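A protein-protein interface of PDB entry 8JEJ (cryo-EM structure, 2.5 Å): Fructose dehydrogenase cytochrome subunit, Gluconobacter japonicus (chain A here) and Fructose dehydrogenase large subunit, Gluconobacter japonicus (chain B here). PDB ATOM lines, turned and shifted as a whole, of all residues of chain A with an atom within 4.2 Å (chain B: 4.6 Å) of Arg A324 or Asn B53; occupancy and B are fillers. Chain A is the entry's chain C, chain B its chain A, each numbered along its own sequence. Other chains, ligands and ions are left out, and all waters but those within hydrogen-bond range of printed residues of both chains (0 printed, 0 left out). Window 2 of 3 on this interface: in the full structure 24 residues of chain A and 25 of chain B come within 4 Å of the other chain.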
ATOM      1  N   VAL A 317      20.299  -6.636 -28.659  1.00  0.00           N
ATOM      2  CA  VAL A 317      19.094  -7.317 -29.118  1.00  0.00           C
ATOM      3  C   VAL A 317      18.913  -8.636 -28.378  1.00  0.00           C
ATOM      4  O   VAL A 317      17.786  -9.046 -28.074  1.00  0.00           O
ATOM      5  CB  VAL A 317      19.148  -7.519 -30.645  1.00  0.00           C
ATOM      6  CG1 VAL A 317      17.933  -8.289 -31.133  1.00  0.00           C
ATOM      7  CG2 VAL A 317      19.242  -6.182 -31.348  1.00  0.00           C
ATOM      8  N   ALA A 320      17.128  -8.639 -24.985  1.00  0.00           N
ATOM      9  CA  ALA A 320      15.692  -8.417 -25.055  1.00  0.00           C
ATOM     10  C   ALA A 320      14.894  -9.708 -25.177  1.00  0.00           C
ATOM     11  O   ALA A 320      13.678  -9.682 -24.962  1.00  0.00           O
ATOM     12  CB  ALA A 320      15.361  -7.497 -26.232  1.00  0.00           C
ATOM     13  N   ASN A 321      15.544 -10.831 -25.501  1.00  0.00           N
ATOM     14  CA  ASN A 321      14.808 -12.070 -25.730  1.00  0.00           C
ATOM     15  C   ASN A 321      14.107 -12.557 -24.471  1.00  0.00           C
ATOM     16  O   ASN A 321      13.027 -13.152 -24.553  1.00  0.00           O
ATOM     17  CB  ASN A 321      15.749 -13.149 -26.261  1.00  0.00           C
ATOM     18  CG  ASN A 321      16.111 -12.935 -27.707  1.00  0.00           C
ATOM     19  OD1 ASN A 321      15.242 -12.726 -28.550  1.00  0.00           O
ATOM     20  ND2 ASN A 321      17.403 -12.976 -28.005  1.00  0.00           N
ATOM     21  N   SER A 322      14.707 -12.328 -23.302  1.00  0.00           N
ATOM     22  CA  SER A 322      14.056 -12.690 -22.052  1.00  0.00           C
ATOM     23  C   SER A 322      12.791 -11.882 -21.804  1.00  0.00           C
ATOM     24  O   SER A 322      11.925 -12.327 -21.044  1.00  0.00           O
ATOM     25  CB  SER A 322      15.024 -12.505 -20.884  1.00  0.00           C
ATOM     26  OG  SER A 322      15.327 -11.135 -20.692  1.00  0.00           O
ATOM     27  N   ARG A 323      12.663 -10.714 -22.428  1.00  0.00           N
ATOM     28  CA  ARG A 323      11.539  -9.821 -22.183  1.00  0.00           C
ATOM     29  C   ARG A 323      10.389 -10.029 -23.156  1.00  0.00           C
ATOM     30  O   ARG A 323       9.431  -9.252 -23.137  1.00  0.00           O
ATOM     31  CB  ARG A 323      12.004  -8.367 -22.225  1.00  0.00           C
ATOM     32  CG  ARG A 323      12.583  -7.890 -20.913  1.00  0.00           C
ATOM     33  CD  ARG A 323      12.922  -6.419 -20.964  1.00  0.00           C
ATOM     34  NE  ARG A 323      13.546  -6.037 -22.224  1.00  0.00           N
ATOM     35  CZ  ARG A 323      14.850  -5.876 -22.390  1.00  0.00           C
ATOM     36  NH1 ARG A 323      15.704  -6.099 -21.407  1.00  0.00           N
ATOM     37  NH2 ARG A 323      15.308  -5.478 -23.573  1.00  0.00           N
ATOM     38  N   ARG A 324      10.469 -11.031 -24.024  1.00  0.00           N
ATOM     39  CA  ARG A 324       9.289 -11.428 -24.770  1.00  0.00           C
ATOM     40  C   ARG A 324       8.304 -12.111 -23.828  1.00  0.00           C
ATOM     41  O   ARG A 324       8.675 -12.616 -22.763  1.00  0.00           O
ATOM     42  CB  ARG A 324       9.671 -12.345 -25.931  1.00  0.00           C
ATOM     43  CG  ARG A 324      10.673 -11.720 -26.889  1.00  0.00           C
ATOM     44  CD  ARG A 324      11.091 -12.690 -27.975  1.00  0.00           C
ATOM     45  NE  ARG A 324      11.704 -13.890 -27.423  1.00  0.00           N
ATOM     46  CZ  ARG A 324      12.344 -14.802 -28.139  1.00  0.00           C
ATOM     47  NH1 ARG A 324      12.471 -14.687 -29.450  1.00  0.00           N
ATOM     48  NH2 ARG A 324      12.872 -15.857 -27.524  1.00  0.00           N
ATOM     49  N   SER A 325       7.030 -12.106 -24.221  1.00  0.00           N
ATOM     50  CA  SER A 325       5.934 -12.552 -23.358  1.00  0.00           C
ATOM     51  C   SER A 325       5.822 -11.687 -22.105  1.00  0.00           C
ATOM     52  O   SER A 325       5.410 -12.161 -21.045  1.00  0.00           O
ATOM     53  CB  SER A 325       6.078 -14.027 -22.971  1.00  0.00           C
ATOM     54  OG  SER A 325       6.926 -14.165 -21.844  1.00  0.00           O
ATOM     55  N   ASN A 326       6.179 -10.411 -22.222  1.00  0.00           N
ATOM     56  CA  ASN A 326       6.247  -9.481 -21.097  1.00  0.00           C
ATOM     57  C   ASN A 326       5.586  -8.158 -21.445  1.00  0.00           C
ATOM     58  O   ASN A 326       6.171  -7.090 -21.265  1.00  0.00           O
ATOM     59  CB  ASN A 326       7.688  -9.230 -20.669  1.00  0.00           C
ATOM     60  CG  ASN A 326       7.974  -9.711 -19.271  1.00  0.00           C
ATOM     61  OD1 ASN A 326       7.069  -9.837 -18.445  1.00  0.00           O
ATOM     62  ND2 ASN A 326       9.242  -9.981 -18.991  1.00  0.00           N
ATOM     63  N   GLU B  49       9.239  -3.942 -29.186  1.00  0.00           N
ATOM     64  CA  GLU B  49      10.412  -4.748 -28.865  1.00  0.00           C
ATOM     65  C   GLU B  49      10.148  -6.231 -29.101  1.00  0.00           C
ATOM     66  O   GLU B  49      11.011  -6.948 -29.620  1.00  0.00           O
ATOM     67  CB  GLU B  49      10.837  -4.508 -27.418  1.00  0.00           C
ATOM     68  CG  GLU B  49      12.127  -5.214 -27.039  1.00  0.00           C
ATOM     69  CD  GLU B  49      12.376  -5.210 -25.548  1.00  0.00           C
ATOM     70  OE1 GLU B  49      11.680  -5.956 -24.828  1.00  0.00           O
ATOM     71  OE2 GLU B  49      13.265  -4.463 -25.095  1.00  0.00           O
ATOM     72  N   ASN B  50       8.960  -6.707 -28.723  1.00  0.00           N
ATOM     73  CA  ASN B  50       8.617  -8.110 -28.926  1.00  0.00           C
ATOM     74  C   ASN B  50       8.591  -8.465 -30.406  1.00  0.00           C
ATOM     75  O   ASN B  50       9.021  -9.557 -30.796  1.00  0.00           O
ATOM     76  CB  ASN B  50       7.264  -8.419 -28.285  1.00  0.00           C
ATOM     77  CG  ASN B  50       7.319  -8.407 -26.775  1.00  0.00           C
ATOM     78  OD1 ASN B  50       8.364  -8.146 -26.182  1.00  0.00           O
ATOM     79  ND2 ASN B  50       6.188  -8.687 -26.142  1.00  0.00           N
ATOM     80  N   TRP B  51       8.071  -7.568 -31.244  1.00  0.00           N
ATOM     81  CA  TRP B  51       8.073  -7.825 -32.679  1.00  0.00           C
ATOM     82  C   TRP B  51       9.486  -7.796 -33.244  1.00  0.00           C
ATOM     83  O   TRP B  51       9.825  -8.604 -34.116  1.00  0.00           O
ATOM     84  CB  TRP B  51       7.191  -6.817 -33.414  1.00  0.00           C
ATOM     85  CG  TRP B  51       7.139  -7.089 -34.886  1.00  0.00           C
ATOM     86  CD1 TRP B  51       6.283  -7.927 -35.532  1.00  0.00           C
ATOM     87  CD2 TRP B  51       8.003  -6.544 -35.892  1.00  0.00           C
ATOM     88  NE1 TRP B  51       6.549  -7.931 -36.879  1.00  0.00           N
ATOM     89  CE2 TRP B  51       7.601  -7.090 -37.126  1.00  0.00           C
ATOM     90  CE3 TRP B  51       9.072  -5.645 -35.869  1.00  0.00           C
ATOM     91  CZ2 TRP B  51       8.230  -6.767 -38.324  1.00  0.00           C
ATOM     92  CZ3 TRP B  51       9.694  -5.325 -37.059  1.00  0.00           C
ATOM     93  CH2 TRP B  51       9.271  -5.883 -38.270  1.00  0.00           C
ATOM     94  N   ARG B  52      10.322  -6.870 -32.770  1.00  0.00           N
ATOM     95  CA  ARG B  52      11.691  -6.791 -33.271  1.00  0.00           C
ATOM     96  C   ARG B  52      12.486  -8.043 -32.931  1.00  0.00           C
ATOM     97  O   ARG B  52      13.337  -8.474 -33.717  1.00  0.00           O
ATOM     98  CB  ARG B  52      12.388  -5.553 -32.713  1.00  0.00           C
ATOM     99  CG  ARG B  52      11.995  -4.258 -33.390  1.00  0.00           C
ATOM    100  CD  ARG B  52      12.251  -3.073 -32.483  1.00  0.00           C
ATOM    101  NE  ARG B  52      12.066  -1.805 -33.177  1.00  0.00           N
ATOM    102  CZ  ARG B  52      12.158  -0.615 -32.603  1.00  0.00           C
ATOM    103  NH1 ARG B  52      12.423  -0.488 -31.314  1.00  0.00           N
ATOM    104  NH2 ARG B  52      11.977   0.477 -33.339  1.00  0.00           N
ATOM    105  N   ASN B  53      12.227  -8.638 -31.770  1.00  0.00           N
ATOM    106  CA  ASN B  53      12.900  -9.854 -31.342  1.00  0.00           C
ATOM    107  C   ASN B  53      12.139 -11.111 -31.735  1.00  0.00           C
ATOM    108  O   ASN B  53      12.489 -12.203 -31.280  1.00  0.00           O
ATOM    109  CB  ASN B  53      13.125  -9.823 -29.830  1.00  0.00           C
ATOM    110  CG  ASN B  53      14.410  -9.122 -29.454  1.00  0.00           C
ATOM    111  OD1 ASN B  53      14.457  -7.896 -29.366  1.00  0.00           O
ATOM    112  ND2 ASN B  53      15.464  -9.896 -29.240  1.00  0.00           N
ATOM    113  N   MET B  54      11.096 -10.975 -32.543  1.00  0.00           N
ATOM    114  CA  MET B  54      10.386 -12.092 -33.145  1.00  0.00           C
ATOM    115  C   MET B  54      11.175 -12.617 -34.344  1.00  0.00           C
ATOM    116  O   MET B  54      11.742 -11.827 -35.102  1.00  0.00           O
ATOM    117  CB  MET B  54       8.988 -11.651 -33.572  1.00  0.00           C
ATOM    118  CG  MET B  54       7.946 -12.752 -33.624  1.00  0.00           C
ATOM    119  SD  MET B  54       6.522 -12.266 -34.610  1.00  0.00           S
ATOM    120  CE  MET B  54       7.327 -11.373 -35.928  1.00  0.00           C
ATOM    121  N   PRO B  55      11.236 -13.935 -34.529  1.00  0.00           N
ATOM    122  CA  PRO B  55      12.129 -14.490 -35.544  1.00  0.00           C
ATOM    123  C   PRO B  55      11.762 -14.006 -36.932  1.00  0.00           C
ATOM    124  O   PRO B  55      10.584 -13.727 -37.224  1.00  0.00           O
ATOM    125  CB  PRO B  55      11.926 -16.004 -35.401  1.00  0.00           C
ATOM    126  CG  PRO B  55      11.531 -16.180 -33.987  1.00  0.00           C
ATOM    127  CD  PRO B  55      10.688 -14.984 -33.653  1.00  0.00           C
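The guanidinium group (NH1) of Arg A324 is in hydrogen-bond range of the backbone carbonyl oxygen (O) of Asn B53 (3.1 Å). The side-chain amide nitrogen of Asn B53 sits at hydrogen-bond distance from the backbone carbonyl oxygen of Val A317, 2.7 Å away. OD1 of Asn A321 lies within hydrogen-bond range of ND2 of Asn B53 (2.9 Å). OE2 of Glu B49 lies within salt-bridge range of NH2 of Arg A323 (2.7 Å). The side-chain amide oxygen (OD1) of Asn B50 lies close to the backbone carbonyl oxygen (O) of Arg A323 (3.4 Å).
Of chain B, only Asn B50 and Asn B53 come within 4 Å of Arg A324. Asn B53 touches just these residues of chain A: Val A317, Ala A320, Asn A321 and Arg A324. Of the printed residues of chain B, Asn A321 touches Asn B53 (2.9 Å). Printed residues of chain A within 4 Å of Glu B49: Ala A320 (3.8 Å) and Arg A323 (2.7 Å). Of the printed residues of chain B, Val A317 touches Asn B53. Printed residues of chain A within 4 Å of Asn B50: Arg A323 (3.4 Å) and Arg A324 (3.7 Å). Printed residues of chain B within 4 Å of Arg A323: Glu B49 and Asn B50. Pro B55 touches none of the printed residues of chain A. Ser A325 touches none of the printed residues of chain B.
The backbone carbonyl oxygen (O) of Asn A321 lies within hydrogen-bond range of the guanidinium group (NE) of Arg A324, at 3.2 Å.
Of the 7 printed residues of chain B, 3 touch a printed residue of chain A. Printed residues of chain B that touch a printed residue of chain A: Glu B49, Asn B50 and Asn B53. Hydrophobic or aromatic side chains of chain A that line the printed part of chain B: Val A317 and Ala A320. Among the printed residues, Asp or Glu carboxylates within 4 Å of a Lys or Arg side-chain nitrogen of the other chain: Arg A323 with Glu B49 (2.7 Å).
Glu B49 touches Ala A320. Ala A320 touches Asn B53 (CB to OD1, 3.3 Å). Arg A324 touches Asn B50 (CA to OD1, 3.7 Å).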
